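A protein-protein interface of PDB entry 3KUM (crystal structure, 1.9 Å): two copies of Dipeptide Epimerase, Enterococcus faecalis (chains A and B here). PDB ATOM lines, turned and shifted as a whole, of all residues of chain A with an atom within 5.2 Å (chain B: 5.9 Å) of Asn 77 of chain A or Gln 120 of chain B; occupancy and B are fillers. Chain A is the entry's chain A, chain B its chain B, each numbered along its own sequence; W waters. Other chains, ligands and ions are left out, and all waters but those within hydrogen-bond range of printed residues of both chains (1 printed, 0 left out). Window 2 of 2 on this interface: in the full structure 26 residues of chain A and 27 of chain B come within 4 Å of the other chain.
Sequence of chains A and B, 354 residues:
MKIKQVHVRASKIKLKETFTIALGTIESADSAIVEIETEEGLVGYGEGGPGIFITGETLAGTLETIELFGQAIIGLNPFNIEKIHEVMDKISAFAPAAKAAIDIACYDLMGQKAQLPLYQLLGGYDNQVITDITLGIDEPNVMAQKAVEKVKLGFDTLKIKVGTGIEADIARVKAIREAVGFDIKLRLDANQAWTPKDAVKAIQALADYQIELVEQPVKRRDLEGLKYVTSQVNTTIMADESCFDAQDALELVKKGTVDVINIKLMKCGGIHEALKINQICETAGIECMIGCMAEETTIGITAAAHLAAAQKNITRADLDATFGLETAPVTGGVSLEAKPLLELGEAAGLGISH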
ATOM      1  N   MET A   1     -18.131   0.917  19.832  1.00  0.00           N
ATOM      2  CA  MET A   1     -17.071   1.863  19.381  1.00  0.00           C
ATOM      3  C   MET A   1     -17.407   2.393  17.987  1.00  0.00           C
ATOM      4  O   MET A   1     -17.840   1.635  17.116  1.00  0.00           O
ATOM      5  CB  MET A   1     -15.721   1.140  19.383  1.00  0.00           C
ATOM      6  CG  MET A   1     -14.533   1.993  19.001  1.00  0.00           C
ATOM      7  SD  MET A   1     -12.976   1.174  19.421  1.00  0.00           S
ATOM      8  CE  MET A   1     -12.399   2.226  20.576  1.00  0.00           C
ATOM      9  N   LYS A   2     -17.222   3.694  17.781  1.00  0.00           N
ATOM     10  CA  LYS A   2     -17.510   4.322  16.494  1.00  0.00           C
ATOM     11  C   LYS A   2     -16.458   5.349  16.118  1.00  0.00           C
ATOM     12  O   LYS A   2     -16.030   6.132  16.955  1.00  0.00           O
ATOM     13  CB  LYS A   2     -18.858   5.048  16.518  1.00  0.00           C
ATOM     14  CG  LYS A   2     -20.082   4.168  16.484  1.00  0.00           C
ATOM     15  CD  LYS A   2     -21.332   5.031  16.314  1.00  0.00           C
ATOM     16  CE  LYS A   2     -22.589   4.175  16.281  1.00  0.00           C
ATOM     17  NZ  LYS A   2     -22.574   3.214  15.144  1.00  0.00           N
ATOM     18  N   ILE A   3     -16.069   5.363  14.850  1.00  0.00           N
ATOM     19  CA  ILE A   3     -15.081   6.323  14.373  1.00  0.00           C
ATOM     20  C   ILE A   3     -15.723   7.705  14.286  1.00  0.00           C
ATOM     21  O   ILE A   3     -16.758   7.881  13.642  1.00  0.00           O
ATOM     22  CB  ILE A   3     -14.525   5.909  12.988  1.00  0.00           C
ATOM     23  CG1 ILE A   3     -13.642   4.666  13.141  1.00  0.00           C
ATOM     24  CG2 ILE A   3     -13.701   7.054  12.367  1.00  0.00           C
ATOM     25  CD1 ILE A   3     -13.283   4.005  11.834  1.00  0.00           C
ATOM     26  N   GLY A  75     -18.264   6.837  11.549  1.00  0.00           N
ATOM     27  CA  GLY A  75     -19.474   6.160  11.976  1.00  0.00           C
ATOM     28  C   GLY A  75     -19.373   4.649  12.041  1.00  0.00           C
ATOM     29  O   GLY A  75     -20.240   3.996  12.621  1.00  0.00           O
ATOM     30  N   LEU A  76     -18.325   4.082  11.446  1.00  0.00           N
ATOM     31  CA  LEU A  76     -18.141   2.633  11.484  1.00  0.00           C
ATOM     32  C   LEU A  76     -17.398   2.221  12.750  1.00  0.00           C
ATOM     33  O   LEU A  76     -16.765   3.044  13.405  1.00  0.00           O
ATOM     34  CB  LEU A  76     -17.358   2.150  10.259  1.00  0.00           C
ATOM     35  CG  LEU A  76     -18.029   2.418   8.910  1.00  0.00           C
ATOM     36  CD1 LEU A  76     -17.208   1.785   7.798  1.00  0.00           C
ATOM     37  CD2 LEU A  76     -19.439   1.855   8.918  1.00  0.00           C
ATOM     38  N   ASN A  77     -17.492   0.941  13.090  1.00  0.00           N
ATOM     39  CA  ASN A  77     -16.823   0.401  14.265  1.00  0.00           C
ATOM     40  C   ASN A  77     -15.460  -0.122  13.800  1.00  0.00           C
ATOM     41  O   ASN A  77     -15.390  -0.850  12.815  1.00  0.00           O
ATOM     42  CB  ASN A  77     -17.647  -0.767  14.832  1.00  0.00           C
ATOM     43  CG  ASN A  77     -17.081  -1.316  16.132  1.00  0.00           C
ATOM     44  OD1 ASN A  77     -15.871  -1.299  16.361  1.00  0.00           O
ATOM     45  ND2 ASN A  77     -17.963  -1.831  16.985  1.00  0.00           N
ATOM     46  N   PRO A  78     -14.367   0.256  14.492  1.00  0.00           N
ATOM     47  CA  PRO A  78     -13.027  -0.209  14.118  1.00  0.00           C
ATOM     48  C   PRO A  78     -12.914  -1.738  14.085  1.00  0.00           C
ATOM     49  O   PRO A  78     -12.053  -2.281  13.386  1.00  0.00           O
ATOM     50  CB  PRO A  78     -12.139   0.426  15.185  1.00  0.00           C
ATOM     51  CG  PRO A  78     -12.824   1.750  15.409  1.00  0.00           C
ATOM     52  CD  PRO A  78     -14.273   1.322  15.508  1.00  0.00           C
ATOM     53  N   PHE A  79     -13.769  -2.428  14.848  1.00  0.00           N
ATOM     54  CA  PHE A  79     -13.761  -3.885  14.871  1.00  0.00           C
ATOM     55  C   PHE A  79     -14.336  -4.496  13.588  1.00  0.00           C
ATOM     56  O   PHE A  79     -14.074  -5.659  13.277  1.00  0.00           O
ATOM     57  CB  PHE A  79     -14.528  -4.398  16.095  1.00  0.00           C
ATOM     58  CG  PHE A  79     -13.736  -4.338  17.368  1.00  0.00           C
ATOM     59  CD1 PHE A  79     -12.741  -5.279  17.624  1.00  0.00           C
ATOM     60  CD2 PHE A  79     -13.966  -3.333  18.300  1.00  0.00           C
ATOM     61  CE1 PHE A  79     -11.984  -5.218  18.794  1.00  0.00           C
ATOM     62  CE2 PHE A  79     -13.215  -3.262  19.469  1.00  0.00           C
ATOM     63  CZ  PHE A  79     -12.221  -4.210  19.714  1.00  0.00           C
ATOM     64  N   ASN A  80     -15.112  -3.714  12.842  1.00  0.00           N
ATOM     65  CA  ASN A  80     -15.689  -4.182  11.575  1.00  0.00           C
ATOM     66  C   ASN A  80     -14.619  -3.965  10.496  1.00  0.00           C
ATOM     67  O   ASN A  80     -14.813  -3.201   9.545  1.00  0.00           O
ATOM     68  CB  ASN A  80     -16.944  -3.368  11.232  1.00  0.00           C
ATOM     69  CG  ASN A  80     -17.783  -4.001  10.125  1.00  0.00           C
ATOM     70  OD1 ASN A  80     -17.359  -4.948   9.456  1.00  0.00           O
ATOM     71  ND2 ASN A  80     -18.992  -3.475   9.933  1.00  0.00           N
ATOM     72  N   ILE A  81     -13.482  -4.632  10.661  1.00  0.00           N
ATOM     73  CA  ILE A  81     -12.379  -4.502   9.722  1.00  0.00           C
ATOM     74  C   ILE A  81     -12.803  -5.055   8.358  1.00  0.00           C
ATOM     75  O   ILE A  81     -12.280  -4.645   7.321  1.00  0.00           O
ATOM     76  CB  ILE A  81     -11.113  -5.242  10.255  1.00  0.00           C
ATOM     77  CG1 ILE A  81      -9.922  -4.992   9.324  1.00  0.00           C
ATOM     78  CG2 ILE A  81     -11.397  -6.733  10.424  1.00  0.00           C
ATOM     79  CD1 ILE A  81      -9.380  -3.562   9.375  1.00  0.00           C
ATOM     80  N   ILE A  84     -14.619  -2.177   6.709  1.00  0.00           N
ATOM     81  CA  ILE A  84     -13.687  -1.093   6.465  1.00  0.00           C
ATOM     82  C   ILE A  84     -12.879  -1.370   5.196  1.00  0.00           C
ATOM     83  O   ILE A  84     -12.691  -0.475   4.374  1.00  0.00           O
ATOM     84  CB  ILE A  84     -12.784  -0.861   7.703  1.00  0.00           C
ATOM     85  CG1 ILE A  84     -13.607  -0.100   8.760  1.00  0.00           C
ATOM     86  CG2 ILE A  84     -11.521  -0.095   7.313  1.00  0.00           C
ATOM     87  CD1 ILE A  84     -12.979   0.013  10.126  1.00  0.00           C
ATOM     88  N   LEU B 116     -15.831  -8.423  24.862  1.00  0.00           N
ATOM     89  CA  LEU B 116     -16.442  -8.206  23.559  1.00  0.00           C
ATOM     90  C   LEU B 116     -17.143  -9.442  23.017  1.00  0.00           C
ATOM     91  O   LEU B 116     -16.696 -10.573  23.239  1.00  0.00           O
ATOM     92  CB  LEU B 116     -15.373  -7.808  22.540  1.00  0.00           C
ATOM     93  CG  LEU B 116     -14.675  -6.462  22.677  1.00  0.00           C
ATOM     94  CD1 LEU B 116     -13.644  -6.345  21.573  1.00  0.00           C
ATOM     95  CD2 LEU B 116     -15.691  -5.333  22.584  1.00  0.00           C
ATOM     96  N   PRO B 117     -18.254  -9.242  22.292  1.00  0.00           N
ATOM     97  CA  PRO B 117     -18.976 -10.380  21.718  1.00  0.00           C
ATOM     98  C   PRO B 117     -17.992 -10.993  20.726  1.00  0.00           C
ATOM     99  O   PRO B 117     -17.246 -10.259  20.065  1.00  0.00           O
ATOM    100  CB  PRO B 117     -20.161  -9.724  21.013  1.00  0.00           C
ATOM    101  CG  PRO B 117     -20.389  -8.491  21.809  1.00  0.00           C
ATOM    102  CD  PRO B 117     -18.983  -7.987  22.054  1.00  0.00           C
ATOM    103  N   LEU B 118     -17.989 -12.316  20.608  1.00  0.00           N
ATOM    104  CA  LEU B 118     -17.049 -12.986  19.719  1.00  0.00           C
ATOM    105  C   LEU B 118     -17.048 -12.478  18.277  1.00  0.00           C
ATOM    106  O   LEU B 118     -15.987 -12.363  17.664  1.00  0.00           O
ATOM    107  CB  LEU B 118     -17.291 -14.500  19.738  1.00  0.00           C
ATOM    108  CG  LEU B 118     -16.290 -15.366  18.957  1.00  0.00           C
ATOM    109  CD1 LEU B 118     -14.865 -15.089  19.419  1.00  0.00           C
ATOM    110  CD2 LEU B 118     -16.630 -16.831  19.166  1.00  0.00           C
ATOM    111  N   TYR B 119     -18.220 -12.160  17.734  1.00  0.00           N
ATOM    112  CA  TYR B 119     -18.276 -11.690  16.351  1.00  0.00           C
ATOM    113  C   TYR B 119     -17.466 -10.409  16.126  1.00  0.00           C
ATOM    114  O   TYR B 119     -17.084 -10.117  14.988  1.00  0.00           O
ATOM    115  CB  TYR B 119     -19.737 -11.497  15.901  1.00  0.00           C
ATOM    116  CG  TYR B 119     -20.469 -10.356  16.565  1.00  0.00           C
ATOM    117  CD1 TYR B 119     -20.216  -9.032  16.199  1.00  0.00           C
ATOM    118  CD2 TYR B 119     -21.422 -10.595  17.554  1.00  0.00           C
ATOM    119  CE1 TYR B 119     -20.892  -7.975  16.797  1.00  0.00           C
ATOM    120  CE2 TYR B 119     -22.107  -9.539  18.163  1.00  0.00           C
ATOM    121  CZ  TYR B 119     -21.834  -8.234  17.775  1.00  0.00           C
ATOM    122  OH  TYR B 119     -22.505  -7.183  18.353  1.00  0.00           O
ATOM    123  N   GLN B 120     -17.197  -9.654  17.197  1.00  0.00           N
ATOM    124  CA  GLN B 120     -16.411  -8.422  17.079  1.00  0.00           C
ATOM    125  C   GLN B 120     -14.922  -8.740  16.923  1.00  0.00           C
ATOM    126  O   GLN B 120     -14.182  -7.987  16.290  1.00  0.00           O
ATOM    127  CB  GLN B 120     -16.613  -7.506  18.299  1.00  0.00           C
ATOM    128  CG  GLN B 120     -18.001  -6.894  18.406  1.00  0.00           C
ATOM    129  CD  GLN B 120     -18.289  -5.852  17.337  1.00  0.00           C
ATOM    130  OE1 GLN B 120     -17.656  -5.832  16.283  1.00  0.00           O
ATOM    131  NE2 GLN B 120     -19.269  -4.985  17.603  1.00  0.00           N
ATOM    132  N   LEU B 121     -14.483  -9.854  17.499  1.00  0.00           N
ATOM    133  CA  LEU B 121     -13.081 -10.252  17.394  1.00  0.00           C
ATOM    134  C   LEU B 121     -12.777 -10.992  16.093  1.00  0.00           C
ATOM    135  O   LEU B 121     -11.616 -11.107  15.696  1.00  0.00           O
ATOM    136  CB  LEU B 121     -12.693 -11.174  18.552  1.00  0.00           C
ATOM    137  CG  LEU B 121     -12.645 -10.580  19.957  1.00  0.00           C
ATOM    138  CD1 LEU B 121     -12.285 -11.677  20.943  1.00  0.00           C
ATOM    139  CD2 LEU B 121     -11.633  -9.453  20.005  1.00  0.00           C
ATOM    140  N   LEU B 122     -13.814 -11.502  15.441  1.00  0.00           N
ATOM    141  CA  LEU B 122     -13.627 -12.283  14.228  1.00  0.00           C
ATOM    142  C   LEU B 122     -13.896 -11.610  12.882  1.00  0.00           C
ATOM    143  O   LEU B 122     -13.979 -12.307  11.865  1.00  0.00           O
ATOM    144  CB  LEU B 122     -14.471 -13.557  14.330  1.00  0.00           C
ATOM    145  CG  LEU B 122     -14.215 -14.437  15.559  1.00  0.00           C
ATOM    146  CD1 LEU B 122     -15.228 -15.570  15.607  1.00  0.00           C
ATOM    147  CD2 LEU B 122     -12.797 -14.982  15.499  1.00  0.00           C
ATOM    148  N   GLY B 123     -14.038 -10.284  12.864  1.00  0.00           N
ATOM    149  CA  GLY B 123     -14.298  -9.588  11.609  1.00  0.00           C
ATOM    150  C   GLY B 123     -15.329  -8.476  11.749  1.00  0.00           C
ATOM    151  O   GLY B 123     -15.269  -7.462  11.033  1.00  0.00           O
ATOM    152  N   GLY B 124     -16.270  -8.670  12.671  1.00  0.00           N
ATOM    153  CA  GLY B 124     -17.297  -7.673  12.947  1.00  0.00           C
ATOM    154  C   GLY B 124     -18.207  -7.202  11.819  1.00  0.00           C
ATOM    155  O   GLY B 124     -18.824  -6.133  11.931  1.00  0.00           O
ATOM    156  N   HIS B 306     -21.328 -16.804  15.358  1.00  0.00           N
ATOM    157  CA  HIS B 306     -20.488 -15.631  15.581  1.00  0.00           C
ATOM    158  C   HIS B 306     -19.485 -15.488  14.437  1.00  0.00           C
ATOM    159  O   HIS B 306     -19.204 -14.384  13.985  1.00  0.00           O
ATOM    160  CB  HIS B 306     -19.717 -15.753  16.908  1.00  0.00           C
ATOM    161  CG  HIS B 306     -20.480 -15.257  18.094  1.00  0.00           C
ATOM    162  ND1 HIS B 306     -20.500 -13.929  18.462  1.00  0.00           N
ATOM    163  CD2 HIS B 306     -21.299 -15.900  18.960  1.00  0.00           C
ATOM    164  CE1 HIS B 306     -21.300 -13.773  19.502  1.00  0.00           C
ATOM    165  NE2 HIS B 306     -21.800 -14.955  19.822  1.00  0.00           N
ATOM    166  N   ALA B 310     -19.551 -12.533  11.570  1.00  0.00           N
ATOM    167  CA  ALA B 310     -18.323 -11.754  11.483  1.00  0.00           C
ATOM    168  C   ALA B 310     -17.654 -11.633  10.113  1.00  0.00           C
ATOM    169  O   ALA B 310     -17.087 -10.594   9.800  1.00  0.00           O
ATOM    170  CB  ALA B 310     -17.305 -12.305  12.488  1.00  0.00           C
ATOM    171  N   GLU B 346     -24.910  -8.757  22.873  1.00  0.00           N
ATOM    172  CA  GLU B 346     -23.716  -7.980  23.146  1.00  0.00           C
ATOM    173  C   GLU B 346     -22.951  -8.596  24.302  1.00  0.00           C
ATOM    174  O   GLU B 346     -22.001  -8.008  24.813  1.00  0.00           O
ATOM    175  CB  GLU B 346     -24.101  -6.534  23.467  1.00  0.00           C
ATOM    176  CG  GLU B 346     -24.813  -5.855  22.313  1.00  0.00           C
ATOM    177  CD  GLU B 346     -23.960  -5.824  21.062  1.00  0.00           C
ATOM    178  OE1 GLU B 346     -24.528  -5.842  19.946  1.00  0.00           O
ATOM    179  OE2 GLU B 346     -22.717  -5.773  21.197  1.00  0.00           O
HETATM  180  O   HOH W   1     -12.687  -7.848  14.177  1.00  0.00           O
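The side-chain amide nitrogen of Gln 120 of chain B sits close to the side-chain amide nitrogen of Asn 77 of chain A (3.5 Å).
The backbone carbonyl oxygen of Gly 123 of chain B is in hydrogen-bond range of the backbone NH of Ile 81 of chain A (3.4 Å).
The backbone carbonyl oxygen (O) of Phe 79 of chain A sits close to the backbone carbonyl oxygen (O) of Gly 123 of chain B, 3.1 Å away.
The backbone carbonyl oxygen (O) of Gly 124 of chain B sits close to the side-chain amide oxygen (OD1) of Asn 80 of chain A, 3.1 Å away.
OD1 of Asn 77 of chain A sits at hydrogen-bond distance from N of Phe 79 of chain A (2.8 Å).
The backbone NH (N) of Gly 124 of chain B is in hydrogen-bond range of the backbone carbonyl oxygen (O) of Tyr 119 of chain B (2.9 Å).
The side-chain amide nitrogen of Asn 77 of chain A sits close to the backbone carbonyl oxygen of Met 1 of chain A, at 3.5 Å.
Phe 79 of chain A touches Leu 116 of chain B.
Phe 79 of chain A touches Gln 120 of chain B (CD1 to O, 3.3 Å).
Gly 124 of chain B touches Phe 79 of chain A.
O of Gly 123 of chain B touches CA of Asn 80 of chain A (3.4 Å).
Of chain A, only Asn 77 (3.5 Å) and Phe 79 (3.3 Å) come within 4 Å of Gln 120 of chain B.
Of the printed residues of chain A, Gly 123 of chain B touches Phe 79 (3.1 Å), Asn 80 (3.4 Å) and Ile 81 (3.4 Å).
Printed residues of chain B within 4 Å of Ile 81 of chain A: Gly 123.
The nearest printed residue of chain B that does not touch Asn 77 of chain A is Gly 124 of chain B (6.2 Å).
Along chain B the printed residues that touch a printed residue of chain A span positions 116 to 124.
Hydrophobic or aromatic side chains of chain A that line the printed part of chain B: Phe 79 and Ile 81.
Among the printed residues, 8 pairs touch across the chains.
No position is printed for both chains.
Of the 8 pairs that touch across the chains among the printed residues, none has its exchanged pair printed and touching as well.
Water W1 lies within hydrogen-bond range of the backbone carbonyl oxygen (O) of Gln 120 of chain B, the backbone carbonyl oxygen (O) of Phe 79 of chain A and the backbone NH (N) of Gly 123 of chain B.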
